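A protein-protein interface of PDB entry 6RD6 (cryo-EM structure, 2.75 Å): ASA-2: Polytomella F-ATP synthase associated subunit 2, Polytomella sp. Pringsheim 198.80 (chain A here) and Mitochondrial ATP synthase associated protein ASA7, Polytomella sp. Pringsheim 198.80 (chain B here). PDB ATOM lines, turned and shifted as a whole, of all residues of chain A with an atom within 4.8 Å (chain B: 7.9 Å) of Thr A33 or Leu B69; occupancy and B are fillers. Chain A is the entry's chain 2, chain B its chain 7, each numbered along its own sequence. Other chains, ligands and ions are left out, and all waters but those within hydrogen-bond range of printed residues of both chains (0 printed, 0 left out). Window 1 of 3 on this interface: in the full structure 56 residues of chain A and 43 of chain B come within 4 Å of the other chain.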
ATOM      1  N   ALA A  29      -4.776  31.448 -29.578  1.00  0.00           N
ATOM      2  CA  ALA A  29      -6.127  30.902 -29.587  1.00  0.00           C
ATOM      3  C   ALA A  29      -6.591  30.518 -28.187  1.00  0.00           C
ATOM      4  O   ALA A  29      -7.759  30.739 -27.839  1.00  0.00           O
ATOM      5  CB  ALA A  29      -6.193  29.693 -30.515  1.00  0.00           C
ATOM      6  N   VAL A  30      -5.694  29.948 -27.377  1.00  0.00           N
ATOM      7  CA  VAL A  30      -6.043  29.564 -26.010  1.00  0.00           C
ATOM      8  C   VAL A  30      -6.355  30.798 -25.169  1.00  0.00           C
ATOM      9  O   VAL A  30      -7.330  30.816 -24.404  1.00  0.00           O
ATOM     10  CB  VAL A  30      -4.913  28.712 -25.404  1.00  0.00           C
ATOM     11  CG1 VAL A  30      -5.028  28.628 -23.912  1.00  0.00           C
ATOM     12  CG2 VAL A  30      -4.962  27.324 -25.973  1.00  0.00           C
ATOM     13  N   ALA A  31      -5.570  31.865 -25.337  1.00  0.00           N
ATOM     14  CA  ALA A  31      -5.860  33.121 -24.659  1.00  0.00           C
ATOM     15  C   ALA A  31      -7.147  33.766 -25.152  1.00  0.00           C
ATOM     16  O   ALA A  31      -7.869  34.358 -24.345  1.00  0.00           O
ATOM     17  CB  ALA A  31      -4.697  34.090 -24.837  1.00  0.00           C
ATOM     18  N   LEU A  32      -7.458  33.648 -26.446  1.00  0.00           N
ATOM     19  CA  LEU A  32      -8.715  34.174 -26.967  1.00  0.00           C
ATOM     20  C   LEU A  32      -9.914  33.416 -26.411  1.00  0.00           C
ATOM     21  O   LEU A  32     -10.987  33.995 -26.212  1.00  0.00           O
ATOM     22  CB  LEU A  32      -8.715  34.109 -28.491  1.00  0.00           C
ATOM     23  CG  LEU A  32      -7.984  35.177 -29.302  1.00  0.00           C
ATOM     24  CD1 LEU A  32      -8.415  35.103 -30.743  1.00  0.00           C
ATOM     25  CD2 LEU A  32      -8.254  36.533 -28.735  1.00  0.00           C
ATOM     26  N   THR A  33      -9.748  32.116 -26.164  1.00  0.00           N
ATOM     27  CA  THR A  33     -10.831  31.338 -25.572  1.00  0.00           C
ATOM     28  C   THR A  33     -10.998  31.656 -24.090  1.00  0.00           C
ATOM     29  O   THR A  33     -12.128  31.804 -23.607  1.00  0.00           O
ATOM     30  CB  THR A  33     -10.573  29.849 -25.788  1.00  0.00           C
ATOM     31  OG1 THR A  33     -10.478  29.594 -27.190  1.00  0.00           O
ATOM     32  CG2 THR A  33     -11.697  29.008 -25.221  1.00  0.00           C
ATOM     33  N   TYR A  34      -9.887  31.788 -23.360  1.00  0.00           N
ATOM     34  CA  TYR A  34      -9.957  32.090 -21.931  1.00  0.00           C
ATOM     35  C   TYR A  34     -10.489  33.492 -21.675  1.00  0.00           C
ATOM     36  O   TYR A  34     -11.157  33.735 -20.664  1.00  0.00           O
ATOM     37  CB  TYR A  34      -8.582  31.939 -21.295  1.00  0.00           C
ATOM     38  CG  TYR A  34      -8.271  30.555 -20.815  1.00  0.00           C
ATOM     39  CD1 TYR A  34      -7.051  29.972 -21.098  1.00  0.00           C
ATOM     40  CD2 TYR A  34      -9.189  29.836 -20.067  1.00  0.00           C
ATOM     41  CE1 TYR A  34      -6.750  28.713 -20.658  1.00  0.00           C
ATOM     42  CE2 TYR A  34      -8.897  28.570 -19.621  1.00  0.00           C
ATOM     43  CZ  TYR A  34      -7.673  28.018 -19.922  1.00  0.00           C
ATOM     44  OH  TYR A  34      -7.352  26.764 -19.488  1.00  0.00           O
ATOM     45  N   LEU A  35     -10.201  34.426 -22.574  1.00  0.00           N
ATOM     46  CA  LEU A  35     -10.757  35.767 -22.481  1.00  0.00           C
ATOM     47  C   LEU A  35     -12.176  35.873 -23.013  1.00  0.00           C
ATOM     48  O   LEU A  35     -12.758  36.960 -22.910  1.00  0.00           O
ATOM     49  CB  LEU A  35      -9.876  36.757 -23.231  1.00  0.00           C
ATOM     50  CG  LEU A  35      -8.773  37.501 -22.491  1.00  0.00           C
ATOM     51  CD1 LEU A  35      -7.677  36.606 -22.001  1.00  0.00           C
ATOM     52  CD2 LEU A  35      -8.222  38.490 -23.466  1.00  0.00           C
ATOM     53  N   GLN A  36     -12.711  34.792 -23.592  1.00  0.00           N
ATOM     54  CA  GLN A  36     -14.089  34.699 -24.089  1.00  0.00           C
ATOM     55  C   GLN A  36     -14.376  35.753 -25.156  1.00  0.00           C
ATOM     56  O   GLN A  36     -15.283  36.577 -25.029  1.00  0.00           O
ATOM     57  CB  GLN A  36     -15.094  34.786 -22.940  1.00  0.00           C
ATOM     58  CG  GLN A  36     -14.889  33.728 -21.885  1.00  0.00           C
ATOM     59  CD  GLN A  36     -15.638  34.036 -20.618  1.00  0.00           C
ATOM     60  OE1 GLN A  36     -16.822  34.370 -20.649  1.00  0.00           O
ATOM     61  NE2 GLN A  36     -14.953  33.937 -19.486  1.00  0.00           N
ATOM     62  N   LYS A  38     -15.791  36.919 -28.441  1.00  0.00           N
ATOM     63  CA  LYS A  38     -16.780  36.550 -29.448  1.00  0.00           C
ATOM     64  C   LYS A  38     -17.089  37.718 -30.374  1.00  0.00           C
ATOM     65  O   LYS A  38     -17.426  37.514 -31.546  1.00  0.00           O
ATOM     66  CB  LYS A  38     -18.057  36.056 -28.774  1.00  0.00           C
ATOM     67  CG  LYS A  38     -17.868  34.844 -27.885  1.00  0.00           C
ATOM     68  CD  LYS A  38     -17.233  33.692 -28.637  1.00  0.00           C
ATOM     69  CE  LYS A  38     -18.271  32.923 -29.418  1.00  0.00           C
ATOM     70  NZ  LYS A  38     -19.341  32.398 -28.536  1.00  0.00           N
ATOM     71  N   TRP A  44     -10.115  36.353 -34.316  1.00  0.00           N
ATOM     72  CA  TRP A  44     -10.223  34.916 -34.524  1.00  0.00           C
ATOM     73  C   TRP A  44      -9.900  34.543 -35.964  1.00  0.00           C
ATOM     74  O   TRP A  44      -9.336  33.476 -36.223  1.00  0.00           O
ATOM     75  CB  TRP A  44     -11.624  34.438 -34.151  1.00  0.00           C
ATOM     76  CG  TRP A  44     -11.762  34.024 -32.724  1.00  0.00           C
ATOM     77  CD1 TRP A  44     -12.495  34.646 -31.764  1.00  0.00           C
ATOM     78  CD2 TRP A  44     -11.155  32.892 -32.096  1.00  0.00           C
ATOM     79  NE1 TRP A  44     -12.386  33.973 -30.576  1.00  0.00           N
ATOM     80  CE2 TRP A  44     -11.565  32.891 -30.753  1.00  0.00           C
ATOM     81  CE3 TRP A  44     -10.307  31.875 -32.540  1.00  0.00           C
ATOM     82  CZ2 TRP A  44     -11.161  31.915 -29.853  1.00  0.00           C
ATOM     83  CZ3 TRP A  44      -9.903  30.911 -31.643  1.00  0.00           C
ATOM     84  CH2 TRP A  44     -10.326  30.938 -30.315  1.00  0.00           C
ATOM     85  N   TRP A  67      -8.424  22.495 -28.828  1.00  0.00           N
ATOM     86  CA  TRP A  67      -9.245  22.787 -27.657  1.00  0.00           C
ATOM     87  C   TRP A  67      -9.814  24.191 -27.725  1.00  0.00           C
ATOM     88  O   TRP A  67     -10.986  24.407 -27.410  1.00  0.00           O
ATOM     89  CB  TRP A  67      -8.438  22.628 -26.364  1.00  0.00           C
ATOM     90  CG  TRP A  67      -9.232  23.044 -25.142  1.00  0.00           C
ATOM     91  CD1 TRP A  67     -10.076  22.264 -24.418  1.00  0.00           C
ATOM     92  CD2 TRP A  67      -9.273  24.346 -24.531  1.00  0.00           C
ATOM     93  NE1 TRP A  67     -10.640  22.988 -23.401  1.00  0.00           N
ATOM     94  CE2 TRP A  67     -10.166  24.271 -23.452  1.00  0.00           C
ATOM     95  CE3 TRP A  67      -8.652  25.567 -24.806  1.00  0.00           C
ATOM     96  CZ2 TRP A  67     -10.444  25.366 -22.641  1.00  0.00           C
ATOM     97  CZ3 TRP A  67      -8.927  26.649 -24.000  1.00  0.00           C
ATOM     98  CH2 TRP A  67      -9.813  26.542 -22.929  1.00  0.00           C
ATOM     99  N   ALA A  68      -8.993  25.160 -28.125  1.00  0.00           N
ATOM    100  CA  ALA A  68      -9.440  26.543 -28.176  1.00  0.00           C
ATOM    101  C   ALA A  68     -10.467  26.773 -29.273  1.00  0.00           C
ATOM    102  O   ALA A  68     -11.411  27.546 -29.080  1.00  0.00           O
ATOM    103  CB  ALA A  68      -8.239  27.451 -28.371  1.00  0.00           C
ATOM    104  N   ILE A  69     -10.310  26.100 -30.412  1.00  0.00           N
ATOM    105  CA  ILE A  69     -11.283  26.198 -31.493  1.00  0.00           C
ATOM    106  C   ILE A  69     -12.603  25.551 -31.090  1.00  0.00           C
ATOM    107  O   ILE A  69     -13.681  26.116 -31.312  1.00  0.00           O
ATOM    108  CB  ILE A  69     -10.696  25.571 -32.773  1.00  0.00           C
ATOM    109  CG1 ILE A  69      -9.652  26.499 -33.385  1.00  0.00           C
ATOM    110  CG2 ILE A  69     -11.766  25.263 -33.799  1.00  0.00           C
ATOM    111  CD1 ILE A  69      -8.848  25.852 -34.469  1.00  0.00           C
ATOM    112  N   THR A  71     -13.725  24.973 -27.997  1.00  0.00           N
ATOM    113  CA  THR A  71     -14.334  25.586 -26.823  1.00  0.00           C
ATOM    114  C   THR A  71     -14.821  26.995 -27.121  1.00  0.00           C
ATOM    115  O   THR A  71     -15.845  27.431 -26.584  1.00  0.00           O
ATOM    116  CB  THR A  71     -13.333  25.596 -25.668  1.00  0.00           C
ATOM    117  OG1 THR A  71     -12.682  24.323 -25.595  1.00  0.00           O
ATOM    118  CG2 THR A  71     -14.029  25.866 -24.350  1.00  0.00           C
ATOM    119  N   GLY A  72     -14.111  27.722 -27.987  1.00  0.00           N
ATOM    120  CA  GLY A  72     -14.510  29.086 -28.287  1.00  0.00           C
ATOM    121  C   GLY A  72     -15.748  29.162 -29.158  1.00  0.00           C
ATOM    122  O   GLY A  72     -16.377  30.216 -29.268  1.00  0.00           O
ATOM    123  N   GLY A  73     -16.115  28.051 -29.786  1.00  0.00           N
ATOM    124  CA  GLY A  73     -17.222  28.041 -30.714  1.00  0.00           C
ATOM    125  C   GLY A  73     -16.882  28.571 -32.081  1.00  0.00           C
ATOM    126  O   GLY A  73     -17.752  29.148 -32.740  1.00  0.00           O
ATOM    127  N   LEU B  15     -19.691  23.358 -36.640  1.00  0.00           N
ATOM    128  CA  LEU B  15     -19.667  22.905 -35.257  1.00  0.00           C
ATOM    129  C   LEU B  15     -21.066  22.490 -34.811  1.00  0.00           C
ATOM    130  O   LEU B  15     -22.060  23.042 -35.275  1.00  0.00           O
ATOM    131  CB  LEU B  15     -19.104  23.999 -34.348  1.00  0.00           C
ATOM    132  CG  LEU B  15     -18.524  23.587 -32.992  1.00  0.00           C
ATOM    133  CD1 LEU B  15     -17.668  22.345 -33.107  1.00  0.00           C
ATOM    134  CD2 LEU B  15     -17.723  24.724 -32.394  1.00  0.00           C
ATOM    135  N   THR B  19     -21.487  21.413 -27.392  1.00  0.00           N
ATOM    136  CA  THR B  19     -20.066  21.145 -27.262  1.00  0.00           C
ATOM    137  C   THR B  19     -19.768  20.854 -25.798  1.00  0.00           C
ATOM    138  O   THR B  19     -20.356  21.468 -24.904  1.00  0.00           O
ATOM    139  CB  THR B  19     -19.237  22.331 -27.768  1.00  0.00           C
ATOM    140  OG1 THR B  19     -19.747  22.758 -29.034  1.00  0.00           O
ATOM    141  CG2 THR B  19     -17.786  21.943 -27.953  1.00  0.00           C
ATOM    142  N   SER B  21     -16.578  20.765 -24.196  1.00  0.00           N
ATOM    143  CA  SER B  21     -15.210  21.120 -23.851  1.00  0.00           C
ATOM    144  C   SER B  21     -15.237  22.408 -23.048  1.00  0.00           C
ATOM    145  O   SER B  21     -16.020  23.313 -23.348  1.00  0.00           O
ATOM    146  CB  SER B  21     -14.350  21.288 -25.100  1.00  0.00           C
ATOM    147  OG  SER B  21     -14.879  22.299 -25.933  1.00  0.00           O
ATOM    148  N   GLY B  22     -14.400  22.480 -22.030  1.00  0.00           N
ATOM    149  CA  GLY B  22     -14.379  23.612 -21.121  1.00  0.00           C
ATOM    150  C   GLY B  22     -13.149  23.566 -20.253  1.00  0.00           C
ATOM    151  O   GLY B  22     -12.046  23.286 -20.730  1.00  0.00           O
ATOM    152  N   PRO B  27      -5.826  23.561 -21.324  1.00  0.00           N
ATOM    153  CA  PRO B  27      -4.406  23.892 -21.140  1.00  0.00           C
ATOM    154  C   PRO B  27      -4.209  24.841 -19.970  1.00  0.00           C
ATOM    155  O   PRO B  27      -5.012  25.748 -19.743  1.00  0.00           O
ATOM    156  CB  PRO B  27      -4.021  24.554 -22.467  1.00  0.00           C
ATOM    157  CG  PRO B  27      -5.306  24.971 -23.071  1.00  0.00           C
ATOM    158  CD  PRO B  27      -6.282  23.927 -22.671  1.00  0.00           C
ATOM    159  N   VAL B  48      -7.467  33.254 -14.576  1.00  0.00           N
ATOM    160  CA  VAL B  48      -6.562  33.249 -15.719  1.00  0.00           C
ATOM    161  C   VAL B  48      -5.795  34.565 -15.731  1.00  0.00           C
ATOM    162  O   VAL B  48      -6.356  35.631 -15.441  1.00  0.00           O
ATOM    163  CB  VAL B  48      -7.309  33.009 -17.043  1.00  0.00           C
ATOM    164  CG1 VAL B  48      -7.810  31.589 -17.102  1.00  0.00           C
ATOM    165  CG2 VAL B  48      -8.485  33.945 -17.198  1.00  0.00           C
ATOM    166  N   VAL B  61     -12.843  33.005 -14.671  1.00  0.00           N
ATOM    167  CA  VAL B  61     -13.701  32.303 -15.618  1.00  0.00           C
ATOM    168  C   VAL B  61     -14.238  31.043 -14.944  1.00  0.00           C
ATOM    169  O   VAL B  61     -13.484  30.281 -14.326  1.00  0.00           O
ATOM    170  CB  VAL B  61     -12.952  32.004 -16.932  1.00  0.00           C
ATOM    171  CG1 VAL B  61     -11.578  31.390 -16.679  1.00  0.00           C
ATOM    172  CG2 VAL B  61     -13.771  31.118 -17.852  1.00  0.00           C
ATOM    173  N   ALA B  63     -16.554  27.341 -15.113  1.00  0.00           N
ATOM    174  CA  ALA B  63     -16.792  26.274 -16.076  1.00  0.00           C
ATOM    175  C   ALA B  63     -18.043  26.560 -16.894  1.00  0.00           C
ATOM    176  O   ALA B  63     -18.099  26.249 -18.091  1.00  0.00           O
ATOM    177  CB  ALA B  63     -16.908  24.931 -15.358  1.00  0.00           C
ATOM    178  N   ALA B  64     -19.044  27.184 -16.270  1.00  0.00           N
ATOM    179  CA  ALA B  64     -20.292  27.490 -16.957  1.00  0.00           C
ATOM    180  C   ALA B  64     -20.109  28.567 -18.015  1.00  0.00           C
ATOM    181  O   ALA B  64     -20.809  28.551 -19.031  1.00  0.00           O
ATOM    182  CB  ALA B  64     -21.355  27.916 -15.949  1.00  0.00           C
ATOM    183  N   ALA B  65     -19.157  29.483 -17.822  1.00  0.00           N
ATOM    184  CA  ALA B  65     -18.894  30.496 -18.839  1.00  0.00           C
ATOM    185  C   ALA B  65     -18.224  29.889 -20.065  1.00  0.00           C
ATOM    186  O   ALA B  65     -18.570  30.228 -21.205  1.00  0.00           O
ATOM    187  CB  ALA B  65     -18.035  31.614 -18.254  1.00  0.00           C
ATOM    188  N   LEU B  66     -17.280  28.967 -19.856  1.00  0.00           N
ATOM    189  CA  LEU B  66     -16.652  28.291 -20.985  1.00  0.00           C
ATOM    190  C   LEU B  66     -17.625  27.347 -21.679  1.00  0.00           C
ATOM    191  O   LEU B  66     -17.485  27.071 -22.875  1.00  0.00           O
ATOM    192  CB  LEU B  66     -15.406  27.533 -20.533  1.00  0.00           C
ATOM    193  CG  LEU B  66     -14.106  28.329 -20.417  1.00  0.00           C
ATOM    194  CD1 LEU B  66     -12.929  27.383 -20.332  1.00  0.00           C
ATOM    195  CD2 LEU B  66     -13.931  29.292 -21.576  1.00  0.00           C
ATOM    196  N   ARG B  67     -18.620  26.842 -20.948  1.00  0.00           N
ATOM    197  CA  ARG B  67     -19.653  26.048 -21.602  1.00  0.00           C
ATOM    198  C   ARG B  67     -20.644  26.934 -22.351  1.00  0.00           C
ATOM    199  O   ARG B  67     -21.224  26.515 -23.358  1.00  0.00           O
ATOM    200  CB  ARG B  67     -20.364  25.173 -20.577  1.00  0.00           C
ATOM    201  CG  ARG B  67     -19.503  24.049 -20.031  1.00  0.00           C
ATOM    202  CD  ARG B  67     -18.986  23.150 -21.133  1.00  0.00           C
ATOM    203  NE  ARG B  67     -20.071  22.606 -21.939  1.00  0.00           N
ATOM    204  CZ  ARG B  67     -20.772  21.526 -21.615  1.00  0.00           C
ATOM    205  NH1 ARG B  67     -20.504  20.866 -20.499  1.00  0.00           N
ATOM    206  NH2 ARG B  67     -21.743  21.102 -22.410  1.00  0.00           N
ATOM    207  N   LYS B  68     -20.846  28.168 -21.880  1.00  0.00           N
ATOM    208  CA  LYS B  68     -21.701  29.109 -22.597  1.00  0.00           C
ATOM    209  C   LYS B  68     -21.008  29.664 -23.832  1.00  0.00           C
ATOM    210  O   LYS B  68     -21.666  30.217 -24.721  1.00  0.00           O
ATOM    211  CB  LYS B  68     -22.094  30.275 -21.692  1.00  0.00           C
ATOM    212  CG  LYS B  68     -23.226  30.036 -20.731  1.00  0.00           C
ATOM    213  CD  LYS B  68     -23.541  31.345 -20.036  1.00  0.00           C
ATOM    214  CE  LYS B  68     -24.646  31.203 -19.022  1.00  0.00           C
ATOM    215  NZ  LYS B  68     -24.207  30.408 -17.844  1.00  0.00           N
ATOM    216  N   LEU B  69     -19.676  29.575 -23.870  1.00  0.00           N
ATOM    217  CA  LEU B  69     -18.902  30.224 -24.927  1.00  0.00           C
ATOM    218  C   LEU B  69     -19.174  29.621 -26.300  1.00  0.00           C
ATOM    219  O   LEU B  69     -19.226  30.343 -27.301  1.00  0.00           O
ATOM    220  CB  LEU B  69     -17.415  30.140 -24.598  1.00  0.00           C
ATOM    221  CG  LEU B  69     -16.547  31.112 -25.380  1.00  0.00           C
ATOM    222  CD1 LEU B  69     -17.011  32.512 -25.100  1.00  0.00           C
ATOM    223  CD2 LEU B  69     -15.101  30.941 -24.997  1.00  0.00           C
ATOM    224  N   SER B  70     -19.368  28.305 -26.371  1.00  0.00           N
ATOM    225  CA  SER B  70     -19.611  27.679 -27.665  1.00  0.00           C
ATOM    226  C   SER B  70     -21.095  27.607 -27.995  1.00  0.00           C
ATOM    227  O   SER B  70     -21.495  26.837 -28.873  1.00  0.00           O
ATOM    228  CB  SER B  70     -18.994  26.286 -27.693  1.00  0.00           C
ATOM    229  OG  SER B  70     -19.633  25.446 -26.756  1.00  0.00           O
ATOM    230  N   GLY B  71     -21.929  28.378 -27.298  1.00  0.00           N
ATOM    231  CA  GLY B  71     -23.343  28.402 -27.628  1.00  0.00           C
ATOM    232  C   GLY B  71     -23.631  29.195 -28.886  1.00  0.00           C
ATOM    233  O   GLY B  71     -24.448  28.789 -29.715  1.00  0.00           O
ATOM    234  N   SER B  72     -22.969  30.338 -29.042  1.00  0.00           N
ATOM    235  CA  SER B  72     -23.090  31.163 -30.244  1.00  0.00           C
ATOM    236  C   SER B  72     -21.849  30.921 -31.089  1.00  0.00           C
ATOM    237  O   SER B  72     -20.720  31.117 -30.643  1.00  0.00           O
ATOM    238  CB  SER B  72     -23.249  32.631 -29.880  1.00  0.00           C
ATOM    239  OG  SER B  72     -23.015  33.457 -31.005  1.00  0.00           O
ATOM    240  N   LYS B  73     -22.056  30.475 -32.323  1.00  0.00           N
ATOM    241  CA  LYS B  73     -20.930  30.110 -33.167  1.00  0.00           C
ATOM    242  C   LYS B  73     -20.382  31.318 -33.912  1.00  0.00           C
ATOM    243  O   LYS B  73     -21.133  32.157 -34.414  1.00  0.00           O
ATOM    244  CB  LYS B  73     -21.345  29.033 -34.164  1.00  0.00           C
ATOM    245  CG  LYS B  73     -21.891  27.785 -33.518  1.00  0.00           C
ATOM    246  CD  LYS B  73     -20.904  27.235 -32.520  1.00  0.00           C
ATOM    247  CE  LYS B  73     -21.334  25.883 -32.028  1.00  0.00           C
ATOM    248  NZ  LYS B  73     -22.726  25.898 -31.514  1.00  0.00           N
ATOM    249  N   ILE B  74     -19.059  31.401 -33.981  1.00  0.00           N
ATOM    250  CA  ILE B  74     -18.376  32.326 -34.873  1.00  0.00           C
ATOM    251  C   ILE B  74     -18.110  31.582 -36.172  1.00  0.00           C
ATOM    252  O   ILE B  74     -17.216  30.731 -36.237  1.00  0.00           O
ATOM    253  CB  ILE B  74     -17.069  32.851 -34.261  1.00  0.00           C
ATOM    254  CG1 ILE B  74     -17.348  33.604 -32.966  1.00  0.00           C
ATOM    255  CG2 ILE B  74     -16.358  33.768 -35.236  1.00  0.00           C
ATOM    256  CD1 ILE B  74     -16.101  34.053 -32.257  1.00  0.00           C
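The side-chain amino group (NZ) of Lys B73 lies within hydrogen-bond range of the backbone carbonyl oxygen (O) of Ser B70, at 3.1 Å.
The backbone carbonyl oxygen of Trp A67 is in hydrogen-bond range of the side-chain hydroxyl of Thr A71 (2.5 Å).
The side-chain hydroxyl of Thr A33 sits at hydrogen-bond distance from the backbone carbonyl oxygen of Ala A29.
The side-chain hydroxyl of Thr A33 sits at hydrogen-bond distance from the backbone carbonyl oxygen of Ala A68 (2.9 Å).
The indole nitrogen (NE1) of Trp A67 lies within hydrogen-bond range of the backbone carbonyl oxygen (O) of Gly B22 (3.0 Å).
The backbone NH of Ile B74 lies within hydrogen-bond range of the backbone carbonyl oxygen of Gly A73 (2.9 Å).
The side-chain hydroxyl (OH) of Tyr A34 lies within hydrogen-bond range of the backbone carbonyl oxygen (O) of Pro B27 (2.6 Å).
The side-chain hydroxyl (OG1) of Thr A71 sits at hydrogen-bond distance from the side-chain hydroxyl (OG) of Ser B21, at 3.0 Å.
The side-chain amino group (NZ) of Lys A38 is in hydrogen-bond range of the backbone carbonyl oxygen (O) of Ser B72, at 2.8 Å.
O of Leu B69 sits close to O of Gly A72 (3.5 Å).
The side-chain amino group of Lys A38 is in hydrogen-bond range of the backbone carbonyl oxygen of Leu B69, 2.4 Å away.
Among the printed residues, pairs that only touch across the chains: Val A30 with Pro B27 (3.8 Å), Thr A33 with Leu B66 (3.7 Å), Thr A33 with Leu B69 (3.4 Å), Tyr A34 with Val B48 (3.7 Å), Gln A36 with Val B61 (3.5 Å), Gln A36 with Ala B65 (3.8 Å), Gln A36 with Leu B69 (3.7 Å), Lys A38 with Ile B74 (3.7 Å), Trp A44 with Ile B74 (3.7 Å), Trp A67 with Pro B27 (3.5 Å), Trp A67 with Leu B66 (3.9 Å), Thr A71 with Gly B22 (3.95 Å), Thr A71 with Leu B66 (3.9 Å), Thr A71 with Leu B69 (3.7 Å), Thr A71 with Ser B70 (3.5 Å), Gly A73 with Leu B15 (3.8 Å), Gly A73 with Ser B70 (3.9 Å) and Gly A73 with Lys B73 (3.3 Å).
Leu A32 touches none of the printed residues of chain B.
Of chain B, only Leu B66 (3.7 Å) and Leu B69 (3.4 Å) come within 4 Å of Thr A33.
Printed residues of chain B within 4 Å of Gln A36: Val B61 (3.5 Å), Ala B65 (3.8 Å) and Leu B69 (3.7 Å).
Printed residues of chain B within 4 Å of Trp A44: Ile B74.
Of the printed residues of chain B, Trp A67 touches Gly B22, Pro B27 and Leu B66.
Printed residues of chain A within 4 Å of Leu B15: Gly A73.
Ala B63 touches none of the printed residues of chain A.
Leu B69 touches five residues of chain A.
Of the printed residues of chain A, Ser B72 touches Lys A38.
The nearest residue of chain A that does not touch Leu B69 is Gly A73 (4.6 Å).
The nearest printed residue of chain B that does not touch Thr A71 is Thr B19 (5.1 Å).
Printed residues of chain B that touch a printed residue of chain A: Leu B15, Ser B21, Gly B22, Pro B27, Val B48, Val B61, Ala B65, Leu B66, Leu B69, Ser B70, Ser B72, Lys B73 and Ile B74.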
